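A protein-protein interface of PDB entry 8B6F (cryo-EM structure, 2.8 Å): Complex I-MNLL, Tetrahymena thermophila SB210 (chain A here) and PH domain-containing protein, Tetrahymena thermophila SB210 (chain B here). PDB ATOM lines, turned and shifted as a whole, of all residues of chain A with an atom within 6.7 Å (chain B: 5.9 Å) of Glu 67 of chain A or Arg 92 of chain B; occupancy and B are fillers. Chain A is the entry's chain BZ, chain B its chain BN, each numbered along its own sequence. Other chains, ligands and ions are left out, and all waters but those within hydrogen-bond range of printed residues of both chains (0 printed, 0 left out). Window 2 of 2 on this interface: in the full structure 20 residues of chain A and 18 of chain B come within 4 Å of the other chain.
Of the 14 printed residues of chain A, 5 touch a printed residue of chain B.
Hydrophobic or aromatic side chains of chain A within 4 Å of the printed part of chain B: Leu 59.
Of the 14 printed residues of chain B, 4 touch a printed residue of chain A.
Among the printed residues, Asp or Glu carboxylates within 4 Å of a Lys or Arg side-chain nitrogen of the other chain: Glu 67 of chain A with Arg 92 of chain B (2.9 Å).
Of the printed residues of chain B, Leu 59 of chain A touches Phe 91.
Of the printed residues of chain B, Cys 60 of chain A touches Arg 92 (3.5 Å).
Of the printed residues of chain B, Glu 64 of chain A touches Arg 92.
Of chain B, only Arg 92 (2.9 Å) and Phe 100 (3.5 Å) come within 4 Å of Glu 67 of chain A.
Arg 68 of chain A touches none of the printed residues of chain B.
Arg 72 of chain A touches none of the printed residues of chain B.
Printed residues of chain A within 4 Å of Pro 90 of chain B: Glu 63.
Of chain A, only Cys 60 (3.5 Å), Glu 63 (2.7 Å), Glu 64 (3.4 Å) and Glu 67 (2.9 Å) come within 4 Å of Arg 92 of chain B.
Printed residues of chain A within 4 Å of Phe 100 of chain B: Glu 67.
The nearest residue of chain B that does not touch Glu 67 of chain A is Pro 90 of chain B (5.5 Å).
The nearest residue of chain A that does not touch Arg 92 of chain B is Tyr 61 of chain A (5.6 Å).
NH2 of Arg 92 of chain B is in salt-bridge range of OD2 of Asp 103 of chain B.
The backbone NH (N) of Phe 91 of chain B is in hydrogen-bond range of the side-chain carboxylate (OE2) of Glu 63 of chain A, at 2.8 Å.
The backbone NH (N) of Arg 92 of chain B lies within hydrogen-bond range of the side-chain carboxylate (OE1) of Glu 63 of chain A, at 2.7 Å.
NH1 of Arg 92 of chain B is in salt-bridge range of OE2 of Glu 67 of chain A (2.9 Å).
Leu 59 of chain A touches Phe 91 of chain B.
Arg 92 of chain B touches Cys 60 of chain A.
Glu 63 of chain A touches Pro 90 of chain B.
CG of Glu 64 of chain A touches NH1 of Arg 92 of chain B, at 3.4 Å.
OE2 of Glu 67 of chain A touches CE1 of Phe 100 of chain B, at 3.5 Å.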
ATOM      1  N   LEU A  59     -18.804  -8.850 -33.605  1.00  0.00           N
ATOM      2  CA  LEU A  59     -19.707  -9.966 -33.347  1.00  0.00           C
ATOM      3  C   LEU A  59     -20.079 -10.039 -31.875  1.00  0.00           C
ATOM      4  O   LEU A  59     -21.244 -10.274 -31.536  1.00  0.00           O
ATOM      5  CB  LEU A  59     -19.062 -11.272 -33.806  1.00  0.00           C
ATOM      6  CG  LEU A  59     -19.740 -12.572 -33.372  1.00  0.00           C
ATOM      7  CD1 LEU A  59     -21.203 -12.605 -33.788  1.00  0.00           C
ATOM      8  CD2 LEU A  59     -18.993 -13.749 -33.965  1.00  0.00           C
ATOM      9  N   CYS A  60     -19.110  -9.828 -30.985  1.00  0.00           N
ATOM     10  CA  CYS A  60     -19.421  -9.804 -29.561  1.00  0.00           C
ATOM     11  C   CYS A  60     -20.415  -8.696 -29.238  1.00  0.00           C
ATOM     12  O   CYS A  60     -21.332  -8.889 -28.432  1.00  0.00           O
ATOM     13  CB  CYS A  60     -18.139  -9.626 -28.750  1.00  0.00           C
ATOM     14  SG  CYS A  60     -17.071 -11.080 -28.727  1.00  0.00           S
ATOM     15  N   TYR A  61     -20.244  -7.523 -29.848  1.00  0.00           N
ATOM     16  CA  TYR A  61     -21.192  -6.435 -29.631  1.00  0.00           C
ATOM     17  C   TYR A  61     -22.562  -6.770 -30.209  1.00  0.00           C
ATOM     18  O   TYR A  61     -23.591  -6.451 -29.604  1.00  0.00           O
ATOM     19  CB  TYR A  61     -20.652  -5.143 -30.239  1.00  0.00           C
ATOM     20  CG  TYR A  61     -19.614  -4.465 -29.375  1.00  0.00           C
ATOM     21  CD1 TYR A  61     -19.976  -3.795 -28.215  1.00  0.00           C
ATOM     22  CD2 TYR A  61     -18.272  -4.494 -29.724  1.00  0.00           C
ATOM     23  CE1 TYR A  61     -19.028  -3.176 -27.425  1.00  0.00           C
ATOM     24  CE2 TYR A  61     -17.318  -3.879 -28.941  1.00  0.00           C
ATOM     25  CZ  TYR A  61     -17.701  -3.222 -27.794  1.00  0.00           C
ATOM     26  OH  TYR A  61     -16.750  -2.608 -27.016  1.00  0.00           O
ATOM     27  N   ASN A  62     -22.598  -7.404 -31.384  1.00  0.00           N
ATOM     28  CA  ASN A  62     -23.879  -7.749 -31.991  1.00  0.00           C
ATOM     29  C   ASN A  62     -24.636  -8.779 -31.166  1.00  0.00           C
ATOM     30  O   ASN A  62     -25.871  -8.765 -31.143  1.00  0.00           O
ATOM     31  CB  ASN A  62     -23.670  -8.284 -33.407  1.00  0.00           C
ATOM     32  CG  ASN A  62     -23.205  -7.219 -34.371  1.00  0.00           C
ATOM     33  OD1 ASN A  62     -23.356  -6.024 -34.116  1.00  0.00           O
ATOM     34  ND2 ASN A  62     -22.643  -7.646 -35.494  1.00  0.00           N
ATOM     35  N   GLU A  63     -23.920  -9.678 -30.490  1.00  0.00           N
ATOM     36  CA  GLU A  63     -24.589 -10.686 -29.679  1.00  0.00           C
ATOM     37  C   GLU A  63     -25.387 -10.056 -28.546  1.00  0.00           C
ATOM     38  O   GLU A  63     -26.388 -10.627 -28.101  1.00  0.00           O
ATOM     39  CB  GLU A  63     -23.563 -11.673 -29.129  1.00  0.00           C
ATOM     40  CG  GLU A  63     -23.036 -12.622 -30.186  1.00  0.00           C
ATOM     41  CD  GLU A  63     -21.990 -13.570 -29.650  1.00  0.00           C
ATOM     42  OE1 GLU A  63     -21.642 -13.458 -28.457  1.00  0.00           O
ATOM     43  OE2 GLU A  63     -21.514 -14.427 -30.421  1.00  0.00           O
ATOM     44  N   GLU A  64     -24.966  -8.885 -28.065  1.00  0.00           N
ATOM     45  CA  GLU A  64     -25.749  -8.184 -27.053  1.00  0.00           C
ATOM     46  C   GLU A  64     -27.129  -7.829 -27.588  1.00  0.00           C
ATOM     47  O   GLU A  64     -28.145  -8.051 -26.921  1.00  0.00           O
ATOM     48  CB  GLU A  64     -25.011  -6.928 -26.594  1.00  0.00           C
ATOM     49  CG  GLU A  64     -23.702  -7.212 -25.887  1.00  0.00           C
ATOM     50  CD  GLU A  64     -22.976  -5.947 -25.480  1.00  0.00           C
ATOM     51  OE1 GLU A  64     -23.292  -4.872 -26.030  1.00  0.00           O
ATOM     52  OE2 GLU A  64     -22.093  -6.027 -24.602  1.00  0.00           O
ATOM     53  N   LYS A  65     -27.185  -7.272 -28.799  1.00  0.00           N
ATOM     54  CA  LYS A  65     -28.476  -6.982 -29.413  1.00  0.00           C
ATOM     55  C   LYS A  65     -29.241  -8.265 -29.695  1.00  0.00           C
ATOM     56  O   LYS A  65     -30.462  -8.324 -29.514  1.00  0.00           O
ATOM     57  CB  LYS A  65     -28.281  -6.188 -30.703  1.00  0.00           C
ATOM     58  CG  LYS A  65     -27.601  -4.846 -30.512  1.00  0.00           C
ATOM     59  CD  LYS A  65     -27.442  -4.123 -31.837  1.00  0.00           C
ATOM     60  CE  LYS A  65     -26.753  -2.782 -31.656  1.00  0.00           C
ATOM     61  NZ  LYS A  65     -26.616  -2.050 -32.946  1.00  0.00           N
ATOM     62  N   LEU A  66     -28.538  -9.306 -30.144  1.00  0.00           N
ATOM     63  CA  LEU A  66     -29.203 -10.558 -30.477  1.00  0.00           C
ATOM     64  C   LEU A  66     -29.835 -11.195 -29.246  1.00  0.00           C
ATOM     65  O   LEU A  66     -30.839 -11.906 -29.363  1.00  0.00           O
ATOM     66  CB  LEU A  66     -28.208 -11.516 -31.132  1.00  0.00           C
ATOM     67  CG  LEU A  66     -28.790 -12.761 -31.804  1.00  0.00           C
ATOM     68  CD1 LEU A  66     -29.762 -12.386 -32.913  1.00  0.00           C
ATOM     69  CD2 LEU A  66     -27.673 -13.629 -32.352  1.00  0.00           C
ATOM     70  N   GLU A  67     -29.262 -10.961 -28.064  1.00  0.00           N
ATOM     71  CA  GLU A  67     -29.903 -11.416 -26.836  1.00  0.00           C
ATOM     72  C   GLU A  67     -31.245 -10.728 -26.633  1.00  0.00           C
ATOM     73  O   GLU A  67     -32.219 -11.362 -26.211  1.00  0.00           O
ATOM     74  CB  GLU A  67     -28.989 -11.166 -25.637  1.00  0.00           C
ATOM     75  CG  GLU A  67     -27.804 -12.113 -25.556  1.00  0.00           C
ATOM     76  CD  GLU A  67     -26.902 -11.815 -24.376  1.00  0.00           C
ATOM     77  OE1 GLU A  67     -27.207 -10.870 -23.620  1.00  0.00           O
ATOM     78  OE2 GLU A  67     -25.887 -12.522 -24.207  1.00  0.00           O
ATOM     79  N   ARG A  68     -31.317  -9.427 -26.924  1.00  0.00           N
ATOM     80  CA  ARG A  68     -32.588  -8.720 -26.810  1.00  0.00           C
ATOM     81  C   ARG A  68     -33.616  -9.296 -27.773  1.00  0.00           C
ATOM     82  O   ARG A  68     -34.791  -9.448 -27.423  1.00  0.00           O
ATOM     83  CB  ARG A  68     -32.387  -7.227 -27.068  1.00  0.00           C
ATOM     84  CG  ARG A  68     -33.594  -6.378 -26.707  1.00  0.00           C
ATOM     85  CD  ARG A  68     -33.422  -4.929 -27.142  1.00  0.00           C
ATOM     86  NE  ARG A  68     -32.194  -4.337 -26.622  1.00  0.00           N
ATOM     87  CZ  ARG A  68     -31.054  -4.247 -27.294  1.00  0.00           C
ATOM     88  NH1 ARG A  68     -30.939  -4.703 -28.531  1.00  0.00           N
ATOM     89  NH2 ARG A  68     -30.000  -3.685 -26.710  1.00  0.00           N
ATOM     90  N   TYR A  69     -33.194  -9.617 -28.997  1.00  0.00           N
ATOM     91  CA  TYR A  69     -34.104 -10.237 -29.953  1.00  0.00           C
ATOM     92  C   TYR A  69     -34.576 -11.599 -29.462  1.00  0.00           C
ATOM     93  O   TYR A  69     -35.760 -11.933 -29.580  1.00  0.00           O
ATOM     94  CB  TYR A  69     -33.424 -10.371 -31.314  1.00  0.00           C
ATOM     95  CG  TYR A  69     -34.215 -11.190 -32.305  1.00  0.00           C
ATOM     96  CD1 TYR A  69     -35.215 -10.611 -33.072  1.00  0.00           C
ATOM     97  CD2 TYR A  69     -33.957 -12.543 -32.477  1.00  0.00           C
ATOM     98  CE1 TYR A  69     -35.940 -11.357 -33.979  1.00  0.00           C
ATOM     99  CE2 TYR A  69     -34.677 -13.297 -33.382  1.00  0.00           C
ATOM    100  CZ  TYR A  69     -35.667 -12.698 -34.129  1.00  0.00           C
ATOM    101  OH  TYR A  69     -36.386 -13.445 -35.032  1.00  0.00           O
ATOM    102  N   GLN A  70     -33.664 -12.401 -28.913  1.00  0.00           N
ATOM    103  CA  GLN A  70     -34.038 -13.735 -28.453  1.00  0.00           C
ATOM    104  C   GLN A  70     -35.081 -13.667 -27.347  1.00  0.00           C
ATOM    105  O   GLN A  70     -36.045 -14.441 -27.345  1.00  0.00           O
ATOM    106  CB  GLN A  70     -32.798 -14.487 -27.970  1.00  0.00           C
ATOM    107  CG  GLN A  70     -31.904 -15.001 -29.084  1.00  0.00           C
ATOM    108  CD  GLN A  70     -32.530 -16.151 -29.846  1.00  0.00           C
ATOM    109  OE1 GLN A  70     -33.501 -15.970 -30.579  1.00  0.00           O
ATOM    110  NE2 GLN A  70     -31.980 -17.346 -29.668  1.00  0.00           N
ATOM    111  N   ILE A  71     -34.903 -12.754 -26.391  1.00  0.00           N
ATOM    112  CA  ILE A  71     -35.848 -12.646 -25.282  1.00  0.00           C
ATOM    113  C   ILE A  71     -37.227 -12.255 -25.798  1.00  0.00           C
ATOM    114  O   ILE A  71     -38.244 -12.842 -25.411  1.00  0.00           O
ATOM    115  CB  ILE A  71     -35.331 -11.646 -24.232  1.00  0.00           C
ATOM    116  CG1 ILE A  71     -34.025 -12.157 -23.619  1.00  0.00           C
ATOM    117  CG2 ILE A  71     -36.376 -11.420 -23.147  1.00  0.00           C
ATOM    118  CD1 ILE A  71     -33.322 -11.152 -22.729  1.00  0.00           C
ATOM    119  N   ARG A  72     -37.283 -11.258 -26.682  1.00  0.00           N
ATOM    120  CA  ARG A  72     -38.567 -10.818 -27.213  1.00  0.00           C
ATOM    121  C   ARG A  72     -39.124 -11.806 -28.225  1.00  0.00           C
ATOM    122  O   ARG A  72     -40.345 -11.970 -28.321  1.00  0.00           O
ATOM    123  CB  ARG A  72     -38.427  -9.433 -27.839  1.00  0.00           C
ATOM    124  CG  ARG A  72     -37.963  -8.376 -26.857  1.00  0.00           C
ATOM    125  CD  ARG A  72     -37.842  -7.015 -27.512  1.00  0.00           C
ATOM    126  NE  ARG A  72     -37.390  -6.005 -26.565  1.00  0.00           N
ATOM    127  CZ  ARG A  72     -37.195  -4.729 -26.864  1.00  0.00           C
ATOM    128  NH1 ARG A  72     -37.402  -4.264 -28.086  1.00  0.00           N
ATOM    129  NH2 ARG A  72     -36.784  -3.895 -25.914  1.00  0.00           N
ATOM    130  N   PRO B  90     -22.657 -18.693 -27.524  1.00  0.00           N
ATOM    131  CA  PRO B  90     -22.288 -17.321 -27.891  1.00  0.00           C
ATOM    132  C   PRO B  90     -20.782 -17.118 -27.835  1.00  0.00           C
ATOM    133  O   PRO B  90     -20.098 -17.643 -26.955  1.00  0.00           O
ATOM    134  CB  PRO B  90     -23.006 -16.463 -26.842  1.00  0.00           C
ATOM    135  CG  PRO B  90     -24.093 -17.314 -26.324  1.00  0.00           C
ATOM    136  CD  PRO B  90     -23.576 -18.714 -26.373  1.00  0.00           C
ATOM    137  N   PHE B  91     -20.270 -16.337 -28.786  1.00  0.00           N
ATOM    138  CA  PHE B  91     -18.868 -15.941 -28.740  1.00  0.00           C
ATOM    139  C   PHE B  91     -18.568 -15.069 -27.530  1.00  0.00           C
ATOM    140  O   PHE B  91     -17.415 -15.011 -27.092  1.00  0.00           O
ATOM    141  CB  PHE B  91     -18.482 -15.218 -30.027  1.00  0.00           C
ATOM    142  CG  PHE B  91     -18.405 -16.120 -31.219  1.00  0.00           C
ATOM    143  CD1 PHE B  91     -19.557 -16.541 -31.861  1.00  0.00           C
ATOM    144  CD2 PHE B  91     -17.181 -16.552 -31.698  1.00  0.00           C
ATOM    145  CE1 PHE B  91     -19.489 -17.372 -32.958  1.00  0.00           C
ATOM    146  CE2 PHE B  91     -17.105 -17.384 -32.795  1.00  0.00           C
ATOM    147  CZ  PHE B  91     -18.261 -17.795 -33.426  1.00  0.00           C
ATOM    148  N   ARG B  92     -19.577 -14.389 -26.984  1.00  0.00           N
ATOM    149  CA  ARG B  92     -19.391 -13.709 -25.708  1.00  0.00           C
ATOM    150  C   ARG B  92     -19.074 -14.701 -24.600  1.00  0.00           C
ATOM    151  O   ARG B  92     -18.319 -14.382 -23.676  1.00  0.00           O
ATOM    152  CB  ARG B  92     -20.641 -12.909 -25.350  1.00  0.00           C
ATOM    153  CG  ARG B  92     -20.771 -11.578 -26.068  1.00  0.00           C
ATOM    154  CD  ARG B  92     -22.051 -10.873 -25.655  1.00  0.00           C
ATOM    155  NE  ARG B  92     -22.100 -10.653 -24.215  1.00  0.00           N
ATOM    156  CZ  ARG B  92     -23.187 -10.295 -23.545  1.00  0.00           C
ATOM    157  NH1 ARG B  92     -24.347 -10.115 -24.153  1.00  0.00           N
ATOM    158  NH2 ARG B  92     -23.107 -10.116 -22.231  1.00  0.00           N
ATOM    159  N   LEU B  93     -19.659 -15.897 -24.657  1.00  0.00           N
ATOM    160  CA  LEU B  93     -19.337 -16.917 -23.667  1.00  0.00           C
ATOM    161  C   LEU B  93     -17.980 -17.554 -23.944  1.00  0.00           C
ATOM    162  O   LEU B  93     -17.245 -17.880 -23.007  1.00  0.00           O
ATOM    163  CB  LEU B  93     -20.434 -17.983 -23.646  1.00  0.00           C
ATOM    164  CG  LEU B  93     -20.248 -19.157 -22.682  1.00  0.00           C
ATOM    165  CD1 LEU B  93     -20.054 -18.670 -21.258  1.00  0.00           C
ATOM    166  CD2 LEU B  93     -21.436 -20.098 -22.768  1.00  0.00           C
ATOM    167  N   ILE B  94     -17.637 -17.748 -25.218  1.00  0.00           N
ATOM    168  CA  ILE B  94     -16.349 -18.348 -25.552  1.00  0.00           C
ATOM    169  C   ILE B  94     -15.213 -17.408 -25.170  1.00  0.00           C
ATOM    170  O   ILE B  94     -14.245 -17.810 -24.513  1.00  0.00           O
ATOM    171  CB  ILE B  94     -16.300 -18.717 -27.046  1.00  0.00           C
ATOM    172  CG1 ILE B  94     -17.479 -19.620 -27.423  1.00  0.00           C
ATOM    173  CG2 ILE B  94     -14.988 -19.411 -27.385  1.00  0.00           C
ATOM    174  CD1 ILE B  94     -17.626 -20.860 -26.565  1.00  0.00           C
ATOM    175  N   TYR B  95     -15.317 -16.143 -25.570  1.00  0.00           N
ATOM    176  CA  TYR B  95     -14.338 -15.118 -25.241  1.00  0.00           C
ATOM    177  C   TYR B  95     -14.951 -14.148 -24.243  1.00  0.00           C
ATOM    178  O   TYR B  95     -16.102 -13.734 -24.396  1.00  0.00           O
ATOM    179  CB  TYR B  95     -13.891 -14.341 -26.485  1.00  0.00           C
ATOM    180  CG  TYR B  95     -13.447 -15.192 -27.648  1.00  0.00           C
ATOM    181  CD1 TYR B  95     -14.369 -15.855 -28.446  1.00  0.00           C
ATOM    182  CD2 TYR B  95     -12.105 -15.297 -27.977  1.00  0.00           C
ATOM    183  CE1 TYR B  95     -13.966 -16.622 -29.519  1.00  0.00           C
ATOM    184  CE2 TYR B  95     -11.690 -16.061 -29.048  1.00  0.00           C
ATOM    185  CZ  TYR B  95     -12.624 -16.721 -29.815  1.00  0.00           C
ATOM    186  OH  TYR B  95     -12.212 -17.480 -30.884  1.00  0.00           O
ATOM    187  N   ARG B  96     -14.178 -13.776 -23.237  1.00  0.00           N
ATOM    188  CA  ARG B  96     -14.645 -12.830 -22.233  1.00  0.00           C
ATOM    189  C   ARG B  96     -15.838 -13.390 -21.467  1.00  0.00           C
ATOM    190  O   ARG B  96     -16.880 -12.729 -21.384  1.00  0.00           O
ATOM    191  CB  ARG B  96     -15.034 -11.496 -22.880  1.00  0.00           C
ATOM    192  CG  ARG B  96     -13.988 -10.918 -23.819  1.00  0.00           C
ATOM    193  CD  ARG B  96     -12.746 -10.498 -23.059  1.00  0.00           C
ATOM    194  NE  ARG B  96     -11.724  -9.939 -23.935  1.00  0.00           N
ATOM    195  CZ  ARG B  96     -10.863 -10.659 -24.640  1.00  0.00           C
ATOM    196  NH1 ARG B  96     -10.890 -11.981 -24.624  1.00  0.00           N
ATOM    197  NH2 ARG B  96      -9.952 -10.037 -25.381  1.00  0.00           N
ATOM    198  N   PRO B  97     -15.737 -14.593 -20.895  1.00  0.00           N
ATOM    199  CA  PRO B  97     -16.876 -15.131 -20.135  1.00  0.00           C
ATOM    200  C   PRO B  97     -17.237 -14.305 -18.913  1.00  0.00           C
ATOM    201  O   PRO B  97     -18.390 -14.360 -18.470  1.00  0.00           O
ATOM    202  CB  PRO B  97     -16.406 -16.539 -19.746  1.00  0.00           C
ATOM    203  CG  PRO B  97     -14.928 -16.479 -19.801  1.00  0.00           C
ATOM    204  CD  PRO B  97     -14.591 -15.516 -20.896  1.00  0.00           C
ATOM    205  N   GLU B  98     -16.294 -13.547 -18.350  1.00  0.00           N
ATOM    206  CA  GLU B  98     -16.596 -12.764 -17.155  1.00  0.00           C
ATOM    207  C   GLU B  98     -17.642 -11.698 -17.448  1.00  0.00           C
ATOM    208  O   GLU B  98     -18.579 -11.505 -16.666  1.00  0.00           O
ATOM    209  CB  GLU B  98     -15.324 -12.119 -16.608  1.00  0.00           C
ATOM    210  CG  GLU B  98     -14.311 -13.098 -16.045  1.00  0.00           C
ATOM    211  CD  GLU B  98     -13.541 -13.836 -17.121  1.00  0.00           C
ATOM    212  OE1 GLU B  98     -13.910 -13.719 -18.307  1.00  0.00           O
ATOM    213  OE2 GLU B  98     -12.560 -14.531 -16.785  1.00  0.00           O
ATOM    214  N   ILE B  99     -17.491 -10.987 -18.566  1.00  0.00           N
ATOM    215  CA  ILE B  99     -18.466  -9.964 -18.936  1.00  0.00           C
ATOM    216  C   ILE B  99     -19.817 -10.603 -19.222  1.00  0.00           C
ATOM    217  O   ILE B  99     -20.869 -10.056 -18.871  1.00  0.00           O
ATOM    218  CB  ILE B  99     -17.953  -9.151 -20.139  1.00  0.00           C
ATOM    219  CG1 ILE B  99     -16.669  -8.409 -19.760  1.00  0.00           C
ATOM    220  CG2 ILE B  99     -19.015  -8.162 -20.612  1.00  0.00           C
ATOM    221  CD1 ILE B  99     -15.944  -7.798 -20.936  1.00  0.00           C
ATOM    222  N   PHE B 100     -19.810 -11.768 -19.871  1.00  0.00           N
ATOM    223  CA  PHE B 100     -21.053 -12.486 -20.132  1.00  0.00           C
ATOM    224  C   PHE B 100     -21.782 -12.799 -18.831  1.00  0.00           C
ATOM    225  O   PHE B 100     -22.988 -12.558 -18.708  1.00  0.00           O
ATOM    226  CB  PHE B 100     -20.746 -13.765 -20.912  1.00  0.00           C
ATOM    227  CG  PHE B 100     -21.962 -14.567 -21.275  1.00  0.00           C
ATOM    228  CD1 PHE B 100     -22.713 -14.241 -22.391  1.00  0.00           C
ATOM    229  CD2 PHE B 100     -22.336 -15.663 -20.519  1.00  0.00           C
ATOM    230  CE1 PHE B 100     -23.826 -14.981 -22.734  1.00  0.00           C
ATOM    231  CE2 PHE B 100     -23.447 -16.408 -20.858  1.00  0.00           C
ATOM    232  CZ  PHE B 100     -24.193 -16.066 -21.967  1.00  0.00           C
ATOM    233  N   LEU B 101     -21.063 -13.344 -17.848  1.00  0.00           N
ATOM    234  CA  LEU B 101     -21.686 -13.684 -16.574  1.00  0.00           C
ATOM    235  C   LEU B 101     -22.178 -12.442 -15.841  1.00  0.00           C
ATOM    236  O   LEU B 101     -23.267 -12.451 -15.254  1.00  0.00           O
ATOM    237  CB  LEU B 101     -20.698 -14.462 -15.704  1.00  0.00           C
ATOM    238  CG  LEU B 101     -20.291 -15.838 -16.235  1.00  0.00           C
ATOM    239  CD1 LEU B 101     -19.195 -16.435 -15.373  1.00  0.00           C
ATOM    240  CD2 LEU B 101     -21.484 -16.774 -16.297  1.00  0.00           C
ATOM    241  N   ASP B 103     -23.108  -9.512 -17.132  1.00  0.00           N
ATOM    242  CA  ASP B 103     -24.319  -9.042 -17.796  1.00  0.00           C
ATOM    243  C   ASP B 103     -25.510  -9.912 -17.423  1.00  0.00           C
ATOM    244  O   ASP B 103     -26.608  -9.406 -17.165  1.00  0.00           O
ATOM    245  CB  ASP B 103     -24.130  -9.041 -19.314  1.00  0.00           C
ATOM    246  CG  ASP B 103     -23.114  -8.019 -19.778  1.00  0.00           C
ATOM    247  OD1 ASP B 103     -23.023  -6.943 -19.152  1.00  0.00           O
ATOM    248  OD2 ASP B 103     -22.405  -8.289 -20.769  1.00  0.00           O
ATOM    249  N   GLN B 104     -25.306 -11.227 -17.389  1.00  0.00           N
ATOM    250  CA  GLN B 104     -26.361 -12.144 -16.981  1.00  0.00           C
ATOM    251  C   GLN B 104     -26.823 -11.869 -15.556  1.00  0.00           C
ATOM    252  O   GLN B 104     -28.006 -12.042 -15.243  1.00  0.00           O
ATOM    253  CB  GLN B 104     -25.858 -13.576 -17.128  1.00  0.00           C
ATOM    254  CG  GLN B 104     -26.794 -14.647 -16.631  1.00  0.00           C
ATOM    255  CD  GLN B 104     -26.178 -16.017 -16.781  1.00  0.00           C
ATOM    256  OE1 GLN B 104     -26.103 -16.788 -15.825  1.00  0.00           O
ATOM    257  NE2 GLN B 104     -25.717 -16.322 -17.987  1.00  0.00           N
